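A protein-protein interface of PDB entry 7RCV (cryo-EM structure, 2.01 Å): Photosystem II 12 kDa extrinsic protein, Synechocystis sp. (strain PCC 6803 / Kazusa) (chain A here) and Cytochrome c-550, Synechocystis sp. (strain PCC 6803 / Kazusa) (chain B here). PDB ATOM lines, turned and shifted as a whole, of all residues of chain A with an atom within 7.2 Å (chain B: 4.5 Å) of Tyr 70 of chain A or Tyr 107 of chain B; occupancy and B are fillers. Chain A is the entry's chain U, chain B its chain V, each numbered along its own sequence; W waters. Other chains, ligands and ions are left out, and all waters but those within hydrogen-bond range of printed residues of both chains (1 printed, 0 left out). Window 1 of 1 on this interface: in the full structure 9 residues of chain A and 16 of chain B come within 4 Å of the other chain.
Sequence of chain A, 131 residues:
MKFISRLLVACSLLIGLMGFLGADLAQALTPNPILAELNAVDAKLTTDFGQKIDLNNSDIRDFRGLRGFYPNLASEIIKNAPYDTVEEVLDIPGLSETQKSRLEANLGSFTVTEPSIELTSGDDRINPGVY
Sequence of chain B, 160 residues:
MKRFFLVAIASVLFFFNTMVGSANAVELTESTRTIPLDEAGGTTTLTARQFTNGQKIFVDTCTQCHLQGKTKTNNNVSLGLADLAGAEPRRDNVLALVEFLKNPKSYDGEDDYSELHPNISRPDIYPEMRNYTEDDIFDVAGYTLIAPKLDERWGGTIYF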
ATOM      1  N   ILE A  60      12.111 -10.235   7.593  1.00  0.00           N
ATOM      2  CA  ILE A  60      13.030  -9.115   7.411  1.00  0.00           C
ATOM      3  C   ILE A  60      14.373  -9.390   8.080  1.00  0.00           C
ATOM      4  O   ILE A  60      15.393  -8.801   7.704  1.00  0.00           O
ATOM      5  CB  ILE A  60      12.385  -7.812   7.924  1.00  0.00           C
ATOM      6  CG1 ILE A  60      13.236  -6.600   7.544  1.00  0.00           C
ATOM      7  CG2 ILE A  60      12.156  -7.866   9.428  1.00  0.00           C
ATOM      8  CD1 ILE A  60      12.510  -5.287   7.680  1.00  0.00           C
ATOM      9  N   ARG A  61      14.405 -10.289   9.064  1.00  0.00           N
ATOM     10  CA  ARG A  61      15.681 -10.718   9.623  1.00  0.00           C
ATOM     11  C   ARG A  61      16.512 -11.465   8.593  1.00  0.00           C
ATOM     12  O   ARG A  61      17.745 -11.469   8.675  1.00  0.00           O
ATOM     13  CB  ARG A  61      15.451 -11.603  10.849  1.00  0.00           C
ATOM     14  CG  ARG A  61      15.247 -10.838  12.138  1.00  0.00           C
ATOM     15  CD  ARG A  61      14.647 -11.731  13.202  1.00  0.00           C
ATOM     16  NE  ARG A  61      15.584 -12.756  13.649  1.00  0.00           N
ATOM     17  CZ  ARG A  61      16.516 -12.569  14.578  1.00  0.00           C
ATOM     18  NH1 ARG A  61      17.320 -13.565  14.919  1.00  0.00           N
ATOM     19  NH2 ARG A  61      16.643 -11.389  15.170  1.00  0.00           N
ATOM     20  N   ASP A  62      15.862 -12.099   7.618  1.00  0.00           N
ATOM     21  CA  ASP A  62      16.581 -12.879   6.622  1.00  0.00           C
ATOM     22  C   ASP A  62      17.366 -11.997   5.659  1.00  0.00           C
ATOM     23  O   ASP A  62      18.234 -12.507   4.945  1.00  0.00           O
ATOM     24  CB  ASP A  62      15.596 -13.763   5.856  1.00  0.00           C
ATOM     25  CG  ASP A  62      15.101 -14.943   6.689  1.00  0.00           C
ATOM     26  OD1 ASP A  62      14.067 -15.544   6.333  1.00  0.00           O
ATOM     27  OD2 ASP A  62      15.721 -15.257   7.726  1.00  0.00           O
ATOM     28  N   PHE A  63      17.090 -10.695   5.634  1.00  0.00           N
ATOM     29  CA  PHE A  63      17.776  -9.745   4.772  1.00  0.00           C
ATOM     30  C   PHE A  63      19.029  -9.158   5.407  1.00  0.00           C
ATOM     31  O   PHE A  63      19.747  -8.409   4.741  1.00  0.00           O
ATOM     32  CB  PHE A  63      16.835  -8.597   4.401  1.00  0.00           C
ATOM     33  CG  PHE A  63      15.866  -8.934   3.314  1.00  0.00           C
ATOM     34  CD1 PHE A  63      16.158  -8.649   1.993  1.00  0.00           C
ATOM     35  CD2 PHE A  63      14.654  -9.529   3.614  1.00  0.00           C
ATOM     36  CE1 PHE A  63      15.263  -8.960   0.989  1.00  0.00           C
ATOM     37  CE2 PHE A  63      13.753  -9.839   2.613  1.00  0.00           C
ATOM     38  CZ  PHE A  63      14.059  -9.552   1.302  1.00  0.00           C
ATOM     39  N   ARG A  64      19.299  -9.468   6.677  1.00  0.00           N
ATOM     40  CA  ARG A  64      20.403  -8.819   7.378  1.00  0.00           C
ATOM     41  C   ARG A  64      21.756  -9.214   6.802  1.00  0.00           C
ATOM     42  O   ARG A  64      22.713  -8.436   6.887  1.00  0.00           O
ATOM     43  CB  ARG A  64      20.341  -9.147   8.869  1.00  0.00           C
ATOM     44  CG  ARG A  64      19.351  -8.302   9.640  1.00  0.00           C
ATOM     45  CD  ARG A  64      19.066  -8.883  11.011  1.00  0.00           C
ATOM     46  NE  ARG A  64      18.940 -10.334  10.982  1.00  0.00           N
ATOM     47  CZ  ARG A  64      19.219 -11.127  12.009  1.00  0.00           C
ATOM     48  NH1 ARG A  64      19.074 -12.439  11.893  1.00  0.00           N
ATOM     49  NH2 ARG A  64      19.648 -10.608  13.150  1.00  0.00           N
ATOM     50  N   GLY A  65      21.860 -10.407   6.215  1.00  0.00           N
ATOM     51  CA  GLY A  65      23.099 -10.816   5.580  1.00  0.00           C
ATOM     52  C   GLY A  65      23.518  -9.935   4.423  1.00  0.00           C
ATOM     53  O   GLY A  65      24.717  -9.798   4.164  1.00  0.00           O
ATOM     54  N   LEU A  66      22.560  -9.328   3.727  1.00  0.00           N
ATOM     55  CA  LEU A  66      22.860  -8.472   2.585  1.00  0.00           C
ATOM     56  C   LEU A  66      23.240  -7.090   3.094  1.00  0.00           C
ATOM     57  O   LEU A  66      22.397  -6.368   3.633  1.00  0.00           O
ATOM     58  CB  LEU A  66      21.662  -8.403   1.644  1.00  0.00           C
ATOM     59  CG  LEU A  66      21.213  -9.746   1.076  1.00  0.00           C
ATOM     60  CD1 LEU A  66      20.156  -9.545   0.009  1.00  0.00           C
ATOM     61  CD2 LEU A  66      22.398 -10.524   0.528  1.00  0.00           C
ATOM     62  N   ARG A  67      24.507  -6.724   2.926  1.00  0.00           N
ATOM     63  CA  ARG A  67      25.003  -5.465   3.464  1.00  0.00           C
ATOM     64  C   ARG A  67      24.280  -4.285   2.829  1.00  0.00           C
ATOM     65  O   ARG A  67      24.196  -4.175   1.603  1.00  0.00           O
ATOM     66  CB  ARG A  67      26.508  -5.356   3.234  1.00  0.00           C
ATOM     67  CG  ARG A  67      27.171  -4.216   3.983  1.00  0.00           C
ATOM     68  CD  ARG A  67      28.653  -4.149   3.669  1.00  0.00           C
ATOM     69  NE  ARG A  67      29.314  -5.434   3.879  1.00  0.00           N
ATOM     70  CZ  ARG A  67      29.595  -5.948   5.072  1.00  0.00           C
ATOM     71  NH1 ARG A  67      29.278  -5.284   6.175  1.00  0.00           N
ATOM     72  NH2 ARG A  67      30.198  -7.123   5.163  1.00  0.00           N
ATOM     73  N   GLY A  68      23.763  -3.396   3.673  1.00  0.00           N
ATOM     74  CA  GLY A  68      23.041  -2.231   3.218  1.00  0.00           C
ATOM     75  C   GLY A  68      21.552  -2.419   3.041  1.00  0.00           C
ATOM     76  O   GLY A  68      20.881  -1.496   2.563  1.00  0.00           O
ATOM     77  N   PHE A  69      21.008  -3.574   3.414  1.00  0.00           N
ATOM     78  CA  PHE A  69      19.593  -3.866   3.225  1.00  0.00           C
ATOM     79  C   PHE A  69      18.760  -3.601   4.470  1.00  0.00           C
ATOM     80  O   PHE A  69      17.785  -2.849   4.417  1.00  0.00           O
ATOM     81  CB  PHE A  69      19.415  -5.325   2.794  1.00  0.00           C
ATOM     82  CG  PHE A  69      19.355  -5.513   1.313  1.00  0.00           C
ATOM     83  CD1 PHE A  69      20.477  -5.315   0.533  1.00  0.00           C
ATOM     84  CD2 PHE A  69      18.178  -5.893   0.699  1.00  0.00           C
ATOM     85  CE1 PHE A  69      20.426  -5.491  -0.833  1.00  0.00           C
ATOM     86  CE2 PHE A  69      18.123  -6.068  -0.662  1.00  0.00           C
ATOM     87  CZ  PHE A  69      19.249  -5.868  -1.429  1.00  0.00           C
ATOM     88  N   TYR A  70      19.121  -4.204   5.585  1.00  0.00           N
ATOM     89  CA  TYR A  70      18.310  -4.060   6.783  1.00  0.00           C
ATOM     90  C   TYR A  70      18.648  -2.742   7.467  1.00  0.00           C
ATOM     91  O   TYR A  70      19.830  -2.431   7.649  1.00  0.00           O
ATOM     92  CB  TYR A  70      18.537  -5.234   7.733  1.00  0.00           C
ATOM     93  CG  TYR A  70      17.783  -5.124   9.042  1.00  0.00           C
ATOM     94  CD1 TYR A  70      18.277  -4.372  10.100  1.00  0.00           C
ATOM     95  CD2 TYR A  70      16.560  -5.754   9.204  1.00  0.00           C
ATOM     96  CE1 TYR A  70      17.582  -4.265  11.281  1.00  0.00           C
ATOM     97  CE2 TYR A  70      15.857  -5.651  10.388  1.00  0.00           C
ATOM     98  CZ  TYR A  70      16.374  -4.907  11.421  1.00  0.00           C
ATOM     99  OH  TYR A  70      15.678  -4.799  12.599  1.00  0.00           O
ATOM    100  N   PRO A  71      17.649  -1.952   7.873  1.00  0.00           N
ATOM    101  CA  PRO A  71      16.241  -2.319   7.711  1.00  0.00           C
ATOM    102  C   PRO A  71      15.514  -1.648   6.545  1.00  0.00           C
ATOM    103  O   PRO A  71      14.453  -2.123   6.156  1.00  0.00           O
ATOM    104  CB  PRO A  71      15.631  -1.868   9.033  1.00  0.00           C
ATOM    105  CG  PRO A  71      16.461  -0.689   9.443  1.00  0.00           C
ATOM    106  CD  PRO A  71      17.816  -0.815   8.793  1.00  0.00           C
ATOM    107  N   ASN A  72      16.078  -0.570   6.000  1.00  0.00           N
ATOM    108  CA  ASN A  72      15.319   0.293   5.100  1.00  0.00           C
ATOM    109  C   ASN A  72      14.947  -0.426   3.806  1.00  0.00           C
ATOM    110  O   ASN A  72      13.763  -0.571   3.485  1.00  0.00           O
ATOM    111  CB  ASN A  72      16.114   1.567   4.815  1.00  0.00           C
ATOM    112  CG  ASN A  72      16.137   2.506   5.999  1.00  0.00           C
ATOM    113  OD1 ASN A  72      15.113   2.737   6.639  1.00  0.00           O
ATOM    114  ND2 ASN A  72      17.309   3.043   6.307  1.00  0.00           N
ATOM    115  N   LEU A  73      15.946  -0.878   3.046  1.00  0.00           N
ATOM    116  CA  LEU A  73      15.658  -1.546   1.780  1.00  0.00           C
ATOM    117  C   LEU A  73      14.866  -2.827   1.995  1.00  0.00           C
ATOM    118  O   LEU A  73      13.991  -3.161   1.191  1.00  0.00           O
ATOM    119  CB  LEU A  73      16.956  -1.832   1.029  1.00  0.00           C
ATOM    120  CG  LEU A  73      16.814  -2.121  -0.467  1.00  0.00           C
ATOM    121  CD1 LEU A  73      15.752  -1.233  -1.099  1.00  0.00           C
ATOM    122  CD2 LEU A  73      18.150  -1.941  -1.157  1.00  0.00           C
ATOM    123  N   ALA A  74      15.159  -3.560   3.070  1.00  0.00           N
ATOM    124  CA  ALA A  74      14.418  -4.785   3.351  1.00  0.00           C
ATOM    125  C   ALA A  74      12.947  -4.496   3.621  1.00  0.00           C
ATOM    126  O   ALA A  74      12.063  -5.198   3.115  1.00  0.00           O
ATOM    127  CB  ALA A  74      15.050  -5.512   4.537  1.00  0.00           C
ATOM    128  N   SER A  75      12.668  -3.453   4.405  1.00  0.00           N
ATOM    129  CA  SER A  75      11.286  -3.072   4.670  1.00  0.00           C
ATOM    130  C   SER A  75      10.597  -2.599   3.399  1.00  0.00           C
ATOM    131  O   SER A  75       9.424  -2.910   3.168  1.00  0.00           O
ATOM    132  CB  SER A  75      11.238  -1.987   5.744  1.00  0.00           C
ATOM    133  OG  SER A  75      11.431  -0.701   5.190  1.00  0.00           O
ATOM    134  N   ARG A 102      22.173  -1.487  -5.035  1.00  0.00           N
ATOM    135  CA  ARG A 102      22.307  -2.586  -4.082  1.00  0.00           C
ATOM    136  C   ARG A 102      21.456  -3.783  -4.496  1.00  0.00           C
ATOM    137  O   ARG A 102      21.899  -4.936  -4.405  1.00  0.00           O
ATOM    138  CB  ARG A 102      21.924  -2.108  -2.681  1.00  0.00           C
ATOM    139  CG  ARG A 102      22.954  -1.185  -2.043  1.00  0.00           C
ATOM    140  CD  ARG A 102      23.237  -1.582  -0.608  1.00  0.00           C
ATOM    141  NE  ARG A 102      22.330  -0.929   0.333  1.00  0.00           N
ATOM    142  CZ  ARG A 102      22.423   0.341   0.712  1.00  0.00           C
ATOM    143  NH1 ARG A 102      21.548   0.841   1.576  1.00  0.00           N
ATOM    144  NH2 ARG A 102      23.394   1.111   0.242  1.00  0.00           N
ATOM    145  N   ILE A 126       7.575  -9.219   9.281  1.00  0.00           N
ATOM    146  CA  ILE A 126       8.237  -8.167  10.035  1.00  0.00           C
ATOM    147  C   ILE A 126       8.649  -8.646  11.420  1.00  0.00           C
ATOM    148  O   ILE A 126       9.712  -8.278  11.918  1.00  0.00           O
ATOM    149  CB  ILE A 126       7.320  -6.928  10.128  1.00  0.00           C
ATOM    150  CG1 ILE A 126       7.156  -6.290   8.749  1.00  0.00           C
ATOM    151  CG2 ILE A 126       7.860  -5.929  11.141  1.00  0.00           C
ATOM    152  CD1 ILE A 126       8.465  -6.016   8.052  1.00  0.00           C
ATOM    153  N   ASN B  74      16.357  -4.284  20.586  1.00  0.00           N
ATOM    154  CA  ASN B  74      16.186  -4.739  19.206  1.00  0.00           C
ATOM    155  C   ASN B  74      17.257  -5.791  18.926  1.00  0.00           C
ATOM    156  O   ASN B  74      18.381  -5.440  18.565  1.00  0.00           O
ATOM    157  CB  ASN B  74      16.275  -3.578  18.229  1.00  0.00           C
ATOM    158  CG  ASN B  74      16.094  -4.009  16.787  1.00  0.00           C
ATOM    159  OD1 ASN B  74      15.682  -5.133  16.504  1.00  0.00           O
ATOM    160  ND2 ASN B  74      16.408  -3.113  15.865  1.00  0.00           N
ATOM    161  N   ASN B  76      17.438  -7.856  16.474  1.00  0.00           N
ATOM    162  CA  ASN B  76      17.856  -8.000  15.088  1.00  0.00           C
ATOM    163  C   ASN B  76      19.246  -7.424  14.860  1.00  0.00           C
ATOM    164  O   ASN B  76      19.906  -7.790  13.882  1.00  0.00           O
ATOM    165  CB  ASN B  76      16.851  -7.325  14.159  1.00  0.00           C
ATOM    166  CG  ASN B  76      15.490  -7.977  14.205  1.00  0.00           C
ATOM    167  OD1 ASN B  76      15.309  -9.014  14.838  1.00  0.00           O
ATOM    168  ND2 ASN B  76      14.522  -7.367  13.539  1.00  0.00           N
ATOM    169  N   VAL B  77      19.703  -6.539  15.734  1.00  0.00           N
ATOM    170  CA  VAL B  77      20.994  -5.872  15.591  1.00  0.00           C
ATOM    171  C   VAL B  77      21.747  -6.095  16.898  1.00  0.00           C
ATOM    172  O   VAL B  77      21.685  -5.284  17.825  1.00  0.00           O
ATOM    173  CB  VAL B  77      20.841  -4.381  15.279  1.00  0.00           C
ATOM    174  CG1 VAL B  77      22.184  -3.757  14.972  1.00  0.00           C
ATOM    175  CG2 VAL B  77      19.885  -4.174  14.114  1.00  0.00           C
ATOM    176  N   ALA B  82      29.082 -11.540  13.729  1.00  0.00           N
ATOM    177  CA  ALA B  82      28.417 -11.606  12.432  1.00  0.00           C
ATOM    178  C   ALA B  82      27.528 -10.391  12.203  1.00  0.00           C
ATOM    179  O   ALA B  82      27.522  -9.813  11.111  1.00  0.00           O
ATOM    180  CB  ALA B  82      27.606 -12.896  12.320  1.00  0.00           C
ATOM    181  N   ASP B  83      26.767  -9.990  13.222  1.00  0.00           N
ATOM    182  CA  ASP B  83      25.980  -8.769  13.102  1.00  0.00           C
ATOM    183  C   ASP B  83      26.882  -7.561  12.899  1.00  0.00           C
ATOM    184  O   ASP B  83      26.618  -6.719  12.035  1.00  0.00           O
ATOM    185  CB  ASP B  83      25.102  -8.585  14.338  1.00  0.00           C
ATOM    186  CG  ASP B  83      24.081  -9.689  14.492  1.00  0.00           C
ATOM    187  OD1 ASP B  83      24.355 -10.815  14.031  1.00  0.00           O
ATOM    188  OD2 ASP B  83      23.004  -9.433  15.071  1.00  0.00           O
ATOM    189  N   GLY B  86      28.175  -7.518   9.429  1.00  0.00           N
ATOM    190  CA  GLY B  86      27.157  -7.297   8.422  1.00  0.00           C
ATOM    191  C   GLY B  86      26.671  -5.870   8.295  1.00  0.00           C
ATOM    192  O   GLY B  86      25.949  -5.565   7.343  1.00  0.00           O
ATOM    193  N   ALA B  87      27.042  -4.993   9.225  1.00  0.00           N
ATOM    194  CA  ALA B  87      26.603  -3.609   9.172  1.00  0.00           C
ATOM    195  C   ALA B  87      27.274  -2.882   8.011  1.00  0.00           C
ATOM    196  O   ALA B  87      28.272  -3.336   7.447  1.00  0.00           O
ATOM    197  CB  ALA B  87      26.907  -2.891  10.486  1.00  0.00           C
ATOM    198  N   GLU B  88      26.705  -1.744   7.649  1.00  0.00           N
ATOM    199  CA  GLU B  88      27.213  -0.936   6.543  1.00  0.00           C
ATOM    200  C   GLU B  88      27.664   0.419   7.063  1.00  0.00           C
ATOM    201  O   GLU B  88      26.816   1.228   7.484  1.00  0.00           O
ATOM    202  CB  GLU B  88      26.148  -0.771   5.458  1.00  0.00           C
ATOM    203  CG  GLU B  88      26.393   0.391   4.504  1.00  0.00           C
ATOM    204  CD  GLU B  88      27.498   0.111   3.501  1.00  0.00           C
ATOM    205  OE1 GLU B  88      27.761   0.985   2.651  1.00  0.00           O
ATOM    206  OE2 GLU B  88      28.097  -0.983   3.551  1.00  0.00           O
ATOM    207  N   ARG B  91      31.327  -3.051  11.109  1.00  0.00           N
ATOM    208  CA  ARG B  91      31.661  -2.519  12.421  1.00  0.00           C
ATOM    209  C   ARG B  91      32.509  -3.481  13.240  1.00  0.00           C
ATOM    210  O   ARG B  91      32.705  -3.264  14.437  1.00  0.00           O
ATOM    211  CB  ARG B  91      30.384  -2.150  13.172  1.00  0.00           C
ATOM    212  CG  ARG B  91      29.460  -1.274  12.360  1.00  0.00           C
ATOM    213  CD  ARG B  91      28.281  -0.807  13.175  1.00  0.00           C
ATOM    214  NE  ARG B  91      27.562   0.269  12.507  1.00  0.00           N
ATOM    215  CZ  ARG B  91      26.240   0.386  12.489  1.00  0.00           C
ATOM    216  NH1 ARG B  91      25.482  -0.514  13.102  1.00  0.00           N
ATOM    217  NH2 ARG B  91      25.675   1.402  11.857  1.00  0.00           N
ATOM    218  N   LYS B 105      24.219   5.057  13.680  1.00  0.00           N
ATOM    219  CA  LYS B 105      23.452   4.994  12.448  1.00  0.00           C
ATOM    220  C   LYS B 105      22.644   3.706  12.425  1.00  0.00           C
ATOM    221  O   LYS B 105      22.847   2.803  13.240  1.00  0.00           O
ATOM    222  CB  LYS B 105      24.371   5.065  11.221  1.00  0.00           C
ATOM    223  CG  LYS B 105      25.113   6.379  11.077  1.00  0.00           C
ATOM    224  CD  LYS B 105      24.229   7.479  10.519  1.00  0.00           C
ATOM    225  CE  LYS B 105      23.398   6.964   9.354  1.00  0.00           C
ATOM    226  NZ  LYS B 105      22.942   8.051   8.443  1.00  0.00           N
ATOM    227  N   SER B 106      21.721   3.625  11.474  1.00  0.00           N
ATOM    228  CA  SER B 106      20.994   2.387  11.257  1.00  0.00           C
ATOM    229  C   SER B 106      21.936   1.317  10.709  1.00  0.00           C
ATOM    230  O   SER B 106      23.054   1.595  10.273  1.00  0.00           O
ATOM    231  CB  SER B 106      19.818   2.615  10.311  1.00  0.00           C
ATOM    232  OG  SER B 106      20.261   2.832   8.985  1.00  0.00           O
ATOM    233  N   TYR B 107      21.460   0.070  10.738  1.00  0.00           N
ATOM    234  CA  TYR B 107      22.314  -1.063  10.396  1.00  0.00           C
ATOM    235  C   TYR B 107      22.795  -0.991   8.953  1.00  0.00           C
ATOM    236  O   TYR B 107      23.902  -1.440   8.638  1.00  0.00           O
ATOM    237  CB  TYR B 107      21.564  -2.367  10.646  1.00  0.00           C
ATOM    238  CG  TYR B 107      22.431  -3.595  10.582  1.00  0.00           C
ATOM    239  CD1 TYR B 107      23.417  -3.820  11.529  1.00  0.00           C
ATOM    240  CD2 TYR B 107      22.257  -4.535   9.577  1.00  0.00           C
ATOM    241  CE1 TYR B 107      24.204  -4.942  11.480  1.00  0.00           C
ATOM    242  CE2 TYR B 107      23.041  -5.667   9.521  1.00  0.00           C
ATOM    243  CZ  TYR B 107      24.014  -5.864  10.475  1.00  0.00           C
ATOM    244  OH  TYR B 107      24.797  -6.989  10.425  1.00  0.00           O
ATOM    245  N   ASP B 108      21.975  -0.452   8.061  1.00  0.00           N
ATOM    246  CA  ASP B 108      22.408  -0.201   6.693  1.00  0.00           C
ATOM    247  C   ASP B 108      23.024   1.180   6.512  1.00  0.00           C
ATOM    248  O   ASP B 108      23.206   1.614   5.372  1.00  0.00           O
ATOM    249  CB  ASP B 108      21.243  -0.405   5.719  1.00  0.00           C
ATOM    250  CG  ASP B 108      20.033   0.444   6.051  1.00  0.00           C
ATOM    251  OD1 ASP B 108      20.188   1.606   6.459  1.00  0.00           O
ATOM    252  OD2 ASP B 108      18.904  -0.056   5.871  1.00  0.00           O
ATOM    253  N   GLY B 109      23.343   1.867   7.605  1.00  0.00           N
ATOM    254  CA  GLY B 109      24.036   3.144   7.530  1.00  0.00           C
ATOM    255  C   GLY B 109      23.281   4.230   6.798  1.00  0.00           C
ATOM    256  O   GLY B 109      23.899   5.060   6.121  1.00  0.00           O
HETATM  257  O   HOH W   1      11.956  -9.045  13.105  1.00  0.00           O
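Printed residues of chain A that touch a printed residue of chain B: Arg 61, Arg 64, Arg 67, Gly 68, Phe 69, Tyr 70, Pro 71 and Asn 72.
Hydrophobic or aromatic side chains of chain A that line the printed part of chain B: Tyr 70 and Pro 71.
Of the 14 printed residues of chain B, 9 touch a printed residue of chain A.
Printed residues of chain B that touch a printed residue of chain A: Asn 74, Asn 76, Val 77, Gly 86, Ala 87, Glu 88, Ser 106, Tyr 107 and Asp 108.
Among the printed residues, no Asp or Glu carboxylate lies within 4 Å of a Lys or Arg side-chain nitrogen of the other chain.
Tyr 70 of chain A touches just these residues of chain B: Asn 74, Asn 76, Val 77, Tyr 107 and Asp 108.
Printed residues of chain B within 4 Å of Asn 72 of chain A: Ser 106 and Asp 108.
Of the printed residues of chain A, Glu 88 of chain B touches Arg 67 (3.2 Å) and Gly 68 (3.97 Å).
Lys 105 of chain B touches none of the printed residues of chain A.
Of the printed residues of chain A, Tyr 107 of chain B touches Arg 64 (3.8 Å) and Tyr 70 (3.5 Å).
The nearest printed residue of chain B that does not touch Tyr 70 of chain A is Ser 106 of chain B (5.3 Å).
The nearest printed residue of chain B that does not touch Phe 69 of chain A is Glu 88 of chain B (6.2 Å).
Water W1 bridges O of Ile 126 of chain A (2.7 Å) and ND2 of Asn 76 of chain B (3.1 Å).
The guanidinium group of Arg 91 of chain B lies within hydrogen-bond range of the backbone carbonyl oxygen of Ser 106 of chain B.
The backbone NH (N) of Ala 74 of chain A lies within hydrogen-bond range of the backbone carbonyl oxygen (O) of Phe 69 of chain A, at 3.0 Å.
The guanidinium group (NE) of Arg 64 of chain A sits at hydrogen-bond distance from the backbone carbonyl oxygen (O) of Arg 61 of chain A.
NH1 of Arg 102 of chain A sits at hydrogen-bond distance from O of Gly 68 of chain A, at 2.6 Å.
The side-chain carboxylate (OD1) of Asp 108 of chain B lies within hydrogen-bond range of the side-chain hydroxyl (OG) of Ser 106 of chain B (2.8 Å).
The backbone carbonyl oxygen of Tyr 107 of chain B sits at hydrogen-bond distance from the backbone NH of Glu 88 of chain B, 3.0 Å away.
O of Arg 64 of chain A touches CE2 of Tyr 107 of chain B, 3.8 Å away.
NH1 of Arg 67 of chain A touches C of Gly 86 of chain B, 3.4 Å away.
CD of Arg 67 of chain A touches OE2 of Glu 88 of chain B, 3.2 Å away.
Glu 88 of chain B touches Gly 68 of chain A.
Gly 68 of chain A touches Asp 108 of chain B (O to CB, 3.4 Å).
OH of Tyr 70 of chain A touches ND2 of Asn 74 of chain B (3.7 Å).
Val 77 of chain B touches Tyr 70 of chain A (CG2 to CE1, 3.7 Å).
Tyr 70 of chain A touches Tyr 107 of chain B.
Asn 72 of chain A touches Ser 106 of chain B (ND2 to OG, 3.99 Å).
ND2 of Asn 76 of chain B is in hydrogen-bond range of OH of Tyr 70 of chain A, 3.0 Å away.
The guanidinium group (NH2) of Arg 64 of chain A lies within hydrogen-bond range of the backbone carbonyl oxygen (O) of Asn 76 of chain B (2.9 Å).
N of Pro 71 of chain A lies close to OD2 of Asp 108 of chain B.
The backbone carbonyl oxygen (O) of Phe 69 of chain A lies close to the side-chain carboxylate (OD2) of Asp 108 of chain B.
The side-chain carboxylate (OD2) of Asp 108 of chain B lies within hydrogen-bond range of the backbone NH (N) of Asn 72 of chain A (2.9 Å).
O of Tyr 70 of chain A lies within hydrogen-bond range of N of Asp 108 of chain B (2.9 Å).
The side-chain amide oxygen of Asn 76 of chain B is in hydrogen-bond range of the guanidinium group of Arg 61 of chain A, at 2.7 Å.
NH1 of Arg 67 of chain A sits at hydrogen-bond distance from O of Ala 87 of chain B (2.5 Å).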
